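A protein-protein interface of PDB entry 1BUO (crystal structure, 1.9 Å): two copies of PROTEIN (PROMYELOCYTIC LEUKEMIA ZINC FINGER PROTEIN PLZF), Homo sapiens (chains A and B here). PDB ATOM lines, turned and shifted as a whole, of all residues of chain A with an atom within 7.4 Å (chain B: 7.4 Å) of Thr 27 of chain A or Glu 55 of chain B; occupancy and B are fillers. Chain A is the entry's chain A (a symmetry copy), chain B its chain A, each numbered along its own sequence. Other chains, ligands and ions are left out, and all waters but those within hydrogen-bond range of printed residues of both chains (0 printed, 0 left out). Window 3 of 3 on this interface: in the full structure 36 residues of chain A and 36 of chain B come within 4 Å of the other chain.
SG of Cys 49 of chain B is in hydrogen-bond range of O of Thr 45 of chain B. The backbone carbonyl oxygen (O) of Glu 55 of chain B lies within hydrogen-bond range of a ring nitrogen (ND1) of His 59 of chain B (3.2 Å). The backbone carbonyl oxygen (O) of Met 22 of chain A is in hydrogen-bond range of the backbone NH (N) of Thr 27 of chain A. O of Leu 28 of chain A is in hydrogen-bond range of ND1 of His 43 of chain A, 3.2 Å away.
The side-chain sulfur of Cys 49 of chain B sits at hydrogen-bond distance from the backbone NH of Ala 19 of chain A (3.4 Å).
No position is printed for both chains. Of the 8 pairs that touch across the chains among the printed residues, none has its exchanged pair printed and touching as well.
Thr 27 of chain A touches one residue of chain B. Glu 55 of chain B touches two residues of chain A. No residue of chain B comes within 4 Å of Gly 26 of chain A. Of the printed residues of chain B, Lys 18 of chain A touches Cys 49. Of the printed residues of chain B, His 43 of chain A touches Thr 45. Of the printed residues of chain B, Met 22 of chain A touches Ala 48 (3.8 Å), Cys 49 (3.98 Å) and Glu 55 (3.3 Å). Printed residues of chain A within 4 Å of Thr 45 of chain B: His 43. The nearest residue of chain B that does not touch Thr 27 of chain A is His 59 of chain B (5.4 Å).
Of the 17 printed residues of chain B, 4 touch a printed residue of chain A. Hydrophobic or aromatic side chains of chain A that line the printed part of chain B: Ala 19, Met 22, Leu 28 and His 43. Along chain A the printed residues that touch a printed residue of chain B span positions 18 to 43. Among the printed residues, 8 pairs touch across the chains.
Among the printed residues, pairs that only touch across the chains: Lys 18 of chain A with Cys 49 of chain B (3.5 Å), Met 22 of chain A with Ala 48 of chain B (3.8 Å), Met 22 of chain A with Cys 49 of chain B (3.98 Å), Met 22 of chain A with Glu 55 of chain B (3.3 Å), Thr 27 of chain A with Glu 55 of chain B (3.7 Å), Leu 28 of chain A with Ala 48 of chain B (3.5 Å) and His 43 of chain A with Thr 45 of chain B (3.4 Å).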
ATOM      1  N   LYS A  18      -6.699  19.146  30.090  1.00  0.00           N
ATOM      2  CA  LYS A  18      -7.353  20.073  29.206  1.00  0.00           C
ATOM      3  C   LYS A  18      -6.348  20.940  28.439  1.00  0.00           C
ATOM      4  O   LYS A  18      -6.570  21.373  27.291  1.00  0.00           O
ATOM      5  CB  LYS A  18      -8.255  21.022  30.062  1.00  0.00           C
ATOM      6  CG  LYS A  18      -8.966  22.039  29.200  1.00  0.00           C
ATOM      7  CD  LYS A  18      -9.889  21.366  28.131  1.00  0.00           C
ATOM      8  CE  LYS A  18     -10.836  22.478  27.654  1.00  0.00           C
ATOM      9  NZ  LYS A  18     -11.440  22.232  26.320  1.00  0.00           N
ATOM     10  N   ALA A  19      -5.308  21.391  29.165  1.00  0.00           N
ATOM     11  CA  ALA A  19      -4.276  22.194  28.404  1.00  0.00           C
ATOM     12  C   ALA A  19      -3.705  21.364  27.263  1.00  0.00           C
ATOM     13  O   ALA A  19      -3.403  21.934  26.189  1.00  0.00           O
ATOM     14  CB  ALA A  19      -3.109  22.588  29.370  1.00  0.00           C
ATOM     15  N   GLN A  21      -5.183  18.793  25.626  1.00  0.00           N
ATOM     16  CA  GLN A  21      -6.192  18.853  24.530  1.00  0.00           C
ATOM     17  C   GLN A  21      -6.200  20.207  23.847  1.00  0.00           C
ATOM     18  O   GLN A  21      -6.278  20.295  22.595  1.00  0.00           O
ATOM     19  CB  GLN A  21      -7.598  18.549  25.101  1.00  0.00           C
ATOM     20  CG  GLN A  21      -7.876  17.301  25.940  1.00  0.00           C
ATOM     21  CD  GLN A  21      -9.172  17.525  26.741  1.00  0.00           C
ATOM     22  OE1 GLN A  21     -10.103  18.213  26.247  1.00  0.00           O
ATOM     23  NE2 GLN A  21      -9.358  17.067  27.988  1.00  0.00           N
ATOM     24  N   MET A  22      -6.097  21.401  24.444  1.00  0.00           N
ATOM     25  CA  MET A  22      -6.043  22.679  23.816  1.00  0.00           C
ATOM     26  C   MET A  22      -4.795  22.771  22.917  1.00  0.00           C
ATOM     27  O   MET A  22      -4.892  23.217  21.768  1.00  0.00           O
ATOM     28  CB  MET A  22      -6.015  23.881  24.788  1.00  0.00           C
ATOM     29  CG  MET A  22      -7.369  23.954  25.603  1.00  0.00           C
ATOM     30  SD  MET A  22      -7.361  25.563  26.539  1.00  0.00           S
ATOM     31  CE  MET A  22      -9.019  26.064  26.369  1.00  0.00           C
ATOM     32  N   ARG A  23      -3.645  22.347  23.441  1.00  0.00           N
ATOM     33  CA  ARG A  23      -2.433  22.423  22.581  1.00  0.00           C
ATOM     34  C   ARG A  23      -2.625  21.600  21.292  1.00  0.00           C
ATOM     35  O   ARG A  23      -2.291  22.112  20.199  1.00  0.00           O
ATOM     36  CB  ARG A  23      -1.274  21.822  23.368  1.00  0.00           C
ATOM     37  CG  ARG A  23       0.012  21.579  22.548  1.00  0.00           C
ATOM     38  CD  ARG A  23       1.049  20.826  23.352  1.00  0.00           C
ATOM     39  NE  ARG A  23       0.782  19.399  23.593  1.00  0.00           N
ATOM     40  CZ  ARG A  23       1.207  18.438  22.776  1.00  0.00           C
ATOM     41  NH1 ARG A  23       1.847  18.722  21.642  1.00  0.00           N
ATOM     42  NH2 ARG A  23       0.963  17.189  23.150  1.00  0.00           N
ATOM     43  N   LEU A  24      -3.148  20.382  21.420  1.00  0.00           N
ATOM     44  CA  LEU A  24      -3.324  19.580  20.198  1.00  0.00           C
ATOM     45  C   LEU A  24      -4.300  20.206  19.253  1.00  0.00           C
ATOM     46  O   LEU A  24      -4.171  20.060  18.013  1.00  0.00           O
ATOM     47  CB  LEU A  24      -3.678  18.152  20.554  1.00  0.00           C
ATOM     48  CG  LEU A  24      -2.529  17.339  21.178  1.00  0.00           C
ATOM     49  CD1 LEU A  24      -3.152  16.108  21.808  1.00  0.00           C
ATOM     50  CD2 LEU A  24      -1.479  17.121  20.107  1.00  0.00           C
ATOM     51  N   ALA A  25      -5.289  20.985  19.707  1.00  0.00           N
ATOM     52  CA  ALA A  25      -6.202  21.615  18.764  1.00  0.00           C
ATOM     53  C   ALA A  25      -5.711  22.998  18.379  1.00  0.00           C
ATOM     54  O   ALA A  25      -6.387  23.719  17.623  1.00  0.00           O
ATOM     55  CB  ALA A  25      -7.592  21.708  19.437  1.00  0.00           C
ATOM     56  N   GLY A  26      -4.605  23.488  18.930  1.00  0.00           N
ATOM     57  CA  GLY A  26      -4.156  24.855  18.736  1.00  0.00           C
ATOM     58  C   GLY A  26      -4.922  25.897  19.554  1.00  0.00           C
ATOM     59  O   GLY A  26      -4.639  27.106  19.415  1.00  0.00           O
ATOM     60  N   THR A  27      -5.776  25.517  20.509  1.00  0.00           N
ATOM     61  CA  THR A  27      -6.589  26.569  21.180  1.00  0.00           C
ATOM     62  C   THR A  27      -5.821  27.393  22.162  1.00  0.00           C
ATOM     63  O   THR A  27      -5.127  26.727  22.942  1.00  0.00           O
ATOM     64  CB  THR A  27      -7.730  25.833  21.918  1.00  0.00           C
ATOM     65  OG1 THR A  27      -8.309  24.944  20.965  1.00  0.00           O
ATOM     66  CG2 THR A  27      -8.700  26.843  22.530  1.00  0.00           C
ATOM     67  N   LEU A  28      -5.824  28.683  22.163  1.00  0.00           N
ATOM     68  CA  LEU A  28      -5.123  29.616  22.990  1.00  0.00           C
ATOM     69  C   LEU A  28      -3.626  29.543  23.011  1.00  0.00           C
ATOM     70  O   LEU A  28      -2.902  30.102  23.863  1.00  0.00           O
ATOM     71  CB  LEU A  28      -5.601  29.570  24.473  1.00  0.00           C
ATOM     72  CG  LEU A  28      -7.060  29.922  24.663  1.00  0.00           C
ATOM     73  CD1 LEU A  28      -7.452  29.608  26.142  1.00  0.00           C
ATOM     74  CD2 LEU A  28      -7.304  31.374  24.343  1.00  0.00           C
ATOM     75  N   CYS A  29      -3.047  28.909  22.006  1.00  0.00           N
ATOM     76  CA  CYS A  29      -1.572  28.769  21.956  1.00  0.00           C
ATOM     77  C   CYS A  29      -1.016  30.156  21.696  1.00  0.00           C
ATOM     78  O   CYS A  29      -1.631  30.893  20.907  1.00  0.00           O
ATOM     79  CB  CYS A  29      -1.153  27.777  20.890  1.00  0.00           C
ATOM     80  SG  CYS A  29      -1.505  26.072  21.325  1.00  0.00           S
ATOM     81  N   ASP A  30      -0.034  30.608  22.450  1.00  0.00           N
ATOM     82  CA  ASP A  30       0.432  31.980  22.248  1.00  0.00           C
ATOM     83  C   ASP A  30       1.934  32.016  22.012  1.00  0.00           C
ATOM     84  O   ASP A  30       2.529  33.039  22.295  1.00  0.00           O
ATOM     85  CB  ASP A  30       0.089  32.811  23.499  1.00  0.00           C
ATOM     86  CG  ASP A  30       0.612  32.090  24.746  1.00  0.00           C
ATOM     87  OD1 ASP A  30       1.384  31.093  24.660  1.00  0.00           O
ATOM     88  OD2 ASP A  30       0.174  32.458  25.853  1.00  0.00           O
ATOM     89  N   ALA A  42       2.404  26.201  21.477  1.00  0.00           N
ATOM     90  CA  ALA A  42       2.209  25.815  22.851  1.00  0.00           C
ATOM     91  C   ALA A  42       1.737  27.029  23.662  1.00  0.00           C
ATOM     92  O   ALA A  42       1.506  28.058  23.053  1.00  0.00           O
ATOM     93  CB  ALA A  42       3.523  25.409  23.552  1.00  0.00           C
ATOM     94  N   HIS A  43       1.664  26.815  24.991  1.00  0.00           N
ATOM     95  CA  HIS A  43       1.206  27.948  25.806  1.00  0.00           C
ATOM     96  C   HIS A  43       2.334  28.449  26.639  1.00  0.00           C
ATOM     97  O   HIS A  43       2.973  27.587  27.317  1.00  0.00           O
ATOM     98  CB  HIS A  43       0.077  27.445  26.822  1.00  0.00           C
ATOM     99  CG  HIS A  43      -1.045  26.827  26.041  1.00  0.00           C
ATOM    100  ND1 HIS A  43      -2.161  27.473  25.548  1.00  0.00           N
ATOM    101  CD2 HIS A  43      -1.225  25.519  25.778  1.00  0.00           C
ATOM    102  CE1 HIS A  43      -2.929  26.569  24.900  1.00  0.00           C
ATOM    103  NE2 HIS A  43      -2.332  25.392  25.027  1.00  0.00           N
ATOM    104  N   ARG B  44      -4.808  33.357  30.812  1.00  0.00           N
ATOM    105  CA  ARG B  44      -5.912  32.733  30.106  1.00  0.00           C
ATOM    106  C   ARG B  44      -5.955  31.244  30.159  1.00  0.00           C
ATOM    107  O   ARG B  44      -7.052  30.666  30.269  1.00  0.00           O
ATOM    108  CB  ARG B  44      -5.884  33.121  28.607  1.00  0.00           C
ATOM    109  CG  ARG B  44      -6.511  34.482  28.353  1.00  0.00           C
ATOM    110  CD  ARG B  44      -6.007  34.823  26.854  1.00  0.00           C
ATOM    111  NE  ARG B  44      -5.836  36.265  26.988  1.00  0.00           N
ATOM    112  CZ  ARG B  44      -6.834  37.121  26.690  1.00  0.00           C
ATOM    113  NH1 ARG B  44      -8.018  36.756  26.187  1.00  0.00           N
ATOM    114  NH2 ARG B  44      -6.539  38.384  26.997  1.00  0.00           N
ATOM    115  N   THR B  45      -4.803  30.593  29.976  1.00  0.00           N
ATOM    116  CA  THR B  45      -4.849  29.125  29.995  1.00  0.00           C
ATOM    117  C   THR B  45      -5.432  28.628  31.337  1.00  0.00           C
ATOM    118  O   THR B  45      -6.091  27.599  31.245  1.00  0.00           O
ATOM    119  CB  THR B  45      -3.480  28.451  29.748  1.00  0.00           C
ATOM    120  OG1 THR B  45      -2.640  28.930  30.778  1.00  0.00           O
ATOM    121  CG2 THR B  45      -2.951  29.066  28.450  1.00  0.00           C
ATOM    122  N   LEU B  47      -7.468  29.997  33.529  1.00  0.00           N
ATOM    123  CA  LEU B  47      -8.935  30.171  33.606  1.00  0.00           C
ATOM    124  C   LEU B  47      -9.697  29.358  32.585  1.00  0.00           C
ATOM    125  O   LEU B  47     -10.736  28.782  32.915  1.00  0.00           O
ATOM    126  CB  LEU B  47      -9.251  31.654  33.432  1.00  0.00           C
ATOM    127  CG  LEU B  47      -8.710  32.617  34.494  1.00  0.00           C
ATOM    128  CD1 LEU B  47      -9.229  34.034  34.134  1.00  0.00           C
ATOM    129  CD2 LEU B  47      -9.184  32.271  35.900  1.00  0.00           C
ATOM    130  N   ALA B  48      -9.196  29.261  31.348  1.00  0.00           N
ATOM    131  CA  ALA B  48      -9.942  28.438  30.355  1.00  0.00           C
ATOM    132  C   ALA B  48      -9.902  26.992  30.625  1.00  0.00           C
ATOM    133  O   ALA B  48     -10.819  26.213  30.307  1.00  0.00           O
ATOM    134  CB  ALA B  48      -9.392  28.836  28.957  1.00  0.00           C
ATOM    135  N   CYS B  49      -8.884  26.413  31.303  1.00  0.00           N
ATOM    136  CA  CYS B  49      -8.803  25.017  31.617  1.00  0.00           C
ATOM    137  C   CYS B  49      -9.684  24.744  32.866  1.00  0.00           C
ATOM    138  O   CYS B  49     -10.051  23.620  33.013  1.00  0.00           O
ATOM    139  CB  CYS B  49      -7.392  24.494  31.918  1.00  0.00           C
ATOM    140  SG  CYS B  49      -6.548  24.404  30.261  1.00  0.00           S
ATOM    141  N   THR B  50     -10.014  25.728  33.628  1.00  0.00           N
ATOM    142  CA  THR B  50     -10.883  25.537  34.811  1.00  0.00           C
ATOM    143  C   THR B  50     -12.363  25.780  34.463  1.00  0.00           C
ATOM    144  O   THR B  50     -13.181  25.020  35.018  1.00  0.00           O
ATOM    145  CB  THR B  50     -10.467  26.607  35.864  1.00  0.00           C
ATOM    146  OG1 THR B  50      -9.082  26.191  36.258  1.00  0.00           O
ATOM    147  CG2 THR B  50     -11.370  26.442  37.130  1.00  0.00           C
ATOM    148  N   SER B  51     -12.634  26.806  33.684  1.00  0.00           N
ATOM    149  CA  SER B  51     -14.050  27.149  33.389  1.00  0.00           C
ATOM    150  C   SER B  51     -14.330  26.986  31.875  1.00  0.00           C
ATOM    151  O   SER B  51     -13.767  27.758  31.106  1.00  0.00           O
ATOM    152  CB  SER B  51     -14.200  28.616  33.793  1.00  0.00           C
ATOM    153  OG  SER B  51     -15.312  29.265  33.222  1.00  0.00           O
ATOM    154  N   LYS B  52     -15.357  26.204  31.565  1.00  0.00           N
ATOM    155  CA  LYS B  52     -15.753  26.055  30.148  1.00  0.00           C
ATOM    156  C   LYS B  52     -16.239  27.396  29.665  1.00  0.00           C
ATOM    157  O   LYS B  52     -15.977  27.787  28.536  1.00  0.00           O
ATOM    158  CB  LYS B  52     -16.818  24.962  29.918  1.00  0.00           C
ATOM    159  CG  LYS B  52     -16.116  23.625  30.257  1.00  0.00           C
ATOM    160  CD  LYS B  52     -17.084  22.510  30.534  1.00  0.00           C
ATOM    161  CE  LYS B  52     -16.710  21.180  29.916  1.00  0.00           C
ATOM    162  NZ  LYS B  52     -15.649  20.476  30.679  1.00  0.00           N
ATOM    163  N   MET B  53     -16.865  28.180  30.565  1.00  0.00           N
ATOM    164  CA  MET B  53     -17.262  29.528  30.163  1.00  0.00           C
ATOM    165  C   MET B  53     -16.184  30.419  29.779  1.00  0.00           C
ATOM    166  O   MET B  53     -16.237  31.180  28.774  1.00  0.00           O
ATOM    167  CB  MET B  53     -18.223  30.128  31.183  1.00  0.00           C
ATOM    168  CG  MET B  53     -19.021  31.299  30.972  1.00  0.00           C
ATOM    169  SD  MET B  53     -19.856  31.429  29.256  1.00  0.00           S
ATOM    170  CE  MET B  53     -19.233  33.023  29.335  1.00  0.00           C
ATOM    171  N   PHE B  54     -15.028  30.469  30.565  1.00  0.00           N
ATOM    172  CA  PHE B  54     -13.949  31.313  30.129  1.00  0.00           C
ATOM    173  C   PHE B  54     -13.378  30.755  28.815  1.00  0.00           C
ATOM    174  O   PHE B  54     -12.874  31.639  28.132  1.00  0.00           O
ATOM    175  CB  PHE B  54     -12.745  31.399  31.189  1.00  0.00           C
ATOM    176  CG  PHE B  54     -12.960  32.362  32.331  1.00  0.00           C
ATOM    177  CD1 PHE B  54     -13.139  33.713  32.093  1.00  0.00           C
ATOM    178  CD2 PHE B  54     -12.893  31.949  33.701  1.00  0.00           C
ATOM    179  CE1 PHE B  54     -13.324  34.672  33.085  1.00  0.00           C
ATOM    180  CE2 PHE B  54     -13.104  32.890  34.684  1.00  0.00           C
ATOM    181  CZ  PHE B  54     -13.277  34.239  34.397  1.00  0.00           C
ATOM    182  N   GLU B  55     -13.322  29.462  28.614  1.00  0.00           N
ATOM    183  CA  GLU B  55     -12.723  28.910  27.356  1.00  0.00           C
ATOM    184  C   GLU B  55     -13.553  29.439  26.155  1.00  0.00           C
ATOM    185  O   GLU B  55     -12.997  30.059  25.229  1.00  0.00           O
ATOM    186  CB  GLU B  55     -12.849  27.413  27.407  1.00  0.00           C
ATOM    187  CG  GLU B  55     -12.286  26.437  26.414  1.00  0.00           C
ATOM    188  CD  GLU B  55     -12.830  26.519  25.032  1.00  0.00           C
ATOM    189  OE1 GLU B  55     -14.101  26.510  24.960  1.00  0.00           O
ATOM    190  OE2 GLU B  55     -12.080  26.592  24.042  1.00  0.00           O
ATOM    191  N   ILE B  56     -14.890  29.371  26.372  1.00  0.00           N
ATOM    192  CA  ILE B  56     -15.813  29.981  25.385  1.00  0.00           C
ATOM    193  C   ILE B  56     -15.609  31.487  25.368  1.00  0.00           C
ATOM    194  O   ILE B  56     -15.343  31.962  24.214  1.00  0.00           O
ATOM    195  CB  ILE B  56     -17.301  29.656  25.594  1.00  0.00           C
ATOM    196  CG1 ILE B  56     -17.617  28.184  25.491  1.00  0.00           C
ATOM    197  CG2 ILE B  56     -18.168  30.525  24.655  1.00  0.00           C
ATOM    198  CD1 ILE B  56     -18.934  27.742  26.140  1.00  0.00           C
ATOM    199  N   LEU B  57     -15.529  32.282  26.418  1.00  0.00           N
ATOM    200  CA  LEU B  57     -15.417  33.688  26.380  1.00  0.00           C
ATOM    201  C   LEU B  57     -14.223  34.161  25.568  1.00  0.00           C
ATOM    202  O   LEU B  57     -14.159  35.334  25.136  1.00  0.00           O
ATOM    203  CB  LEU B  57     -15.217  34.604  27.599  1.00  0.00           C
ATOM    204  CG  LEU B  57     -16.379  35.023  28.472  1.00  0.00           C
ATOM    205  CD1 LEU B  57     -15.923  35.750  29.734  1.00  0.00           C
ATOM    206  CD2 LEU B  57     -17.403  35.856  27.740  1.00  0.00           C
ATOM    207  N   PHE B  58     -13.079  33.456  25.764  1.00  0.00           N
ATOM    208  CA  PHE B  58     -11.817  33.955  25.200  1.00  0.00           C
ATOM    209  C   PHE B  58     -11.793  33.693  23.689  1.00  0.00           C
ATOM    210  O   PHE B  58     -10.934  34.242  23.009  1.00  0.00           O
ATOM    211  CB  PHE B  58     -10.606  33.227  25.836  1.00  0.00           C
ATOM    212  CG  PHE B  58     -10.410  33.527  27.302  1.00  0.00           C
ATOM    213  CD1 PHE B  58     -10.791  34.730  27.893  1.00  0.00           C
ATOM    214  CD2 PHE B  58      -9.821  32.565  28.105  1.00  0.00           C
ATOM    215  CE1 PHE B  58     -10.603  34.981  29.245  1.00  0.00           C
ATOM    216  CE2 PHE B  58      -9.621  32.806  29.441  1.00  0.00           C
ATOM    217  CZ  PHE B  58      -9.999  33.993  30.051  1.00  0.00           C
ATOM    218  N   HIS B  59     -12.839  33.064  23.154  1.00  0.00           N
ATOM    219  CA  HIS B  59     -13.044  32.866  21.712  1.00  0.00           C
ATOM    220  C   HIS B  59     -12.977  34.237  21.030  1.00  0.00           C
ATOM    221  O   HIS B  59     -12.521  34.369  19.899  1.00  0.00           O
ATOM    222  CB  HIS B  59     -14.394  32.253  21.334  1.00  0.00           C
ATOM    223  CG  HIS B  59     -14.437  30.786  21.553  1.00  0.00           C
ATOM    224  ND1 HIS B  59     -13.398  30.049  22.054  1.00  0.00           N
ATOM    225  CD2 HIS B  59     -15.420  29.892  21.399  1.00  0.00           C
ATOM    226  CE1 HIS B  59     -13.725  28.769  22.122  1.00  0.00           C
ATOM    227  NE2 HIS B  59     -14.991  28.650  21.723  1.00  0.00           N
ATOM    228  N   ARG B  60     -13.400  35.257  21.725  1.00  0.00           N
ATOM    229  CA  ARG B  60     -13.411  36.638  21.322  1.00  0.00           C
ATOM    230  C   ARG B  60     -12.270  37.333  22.024  1.00  0.00           C
ATOM    231  O   ARG B  60     -12.375  37.745  23.172  1.00  0.00           O
ATOM    232  CB  ARG B  60     -14.743  37.269  21.732  1.00  0.00           C
ATOM    233  CG  ARG B  60     -15.464  38.164  20.754  1.00  0.00           C
ATOM    234  CD  ARG B  60     -15.860  39.477  21.413  1.00  0.00           C
ATOM    235  NE  ARG B  60     -17.062  39.388  22.236  1.00  0.00           N
ATOM    236  CZ  ARG B  60     -17.651  40.416  22.851  1.00  0.00           C
ATOM    237  NH1 ARG B  60     -17.118  41.628  22.706  1.00  0.00           N
ATOM    238  NH2 ARG B  60     -18.740  40.271  23.603  1.00  0.00           N
ATOM    239  N   LEU B 104     -20.153  29.800  35.350  1.00  0.00           N
ATOM    240  CA  LEU B 104     -18.791  29.576  34.814  1.00  0.00           C
ATOM    241  C   LEU B 104     -18.618  28.147  34.369  1.00  0.00           C
ATOM    242  O   LEU B 104     -17.530  27.780  33.786  1.00  0.00           O
ATOM    243  CB  LEU B 104     -17.763  29.911  35.952  1.00  0.00           C
ATOM    244  CG  LEU B 104     -17.695  31.409  36.241  1.00  0.00           C
ATOM    245  CD1 LEU B 104     -16.795  31.666  37.496  1.00  0.00           C
ATOM    246  CD2 LEU B 104     -17.054  32.086  35.026  1.00  0.00           C
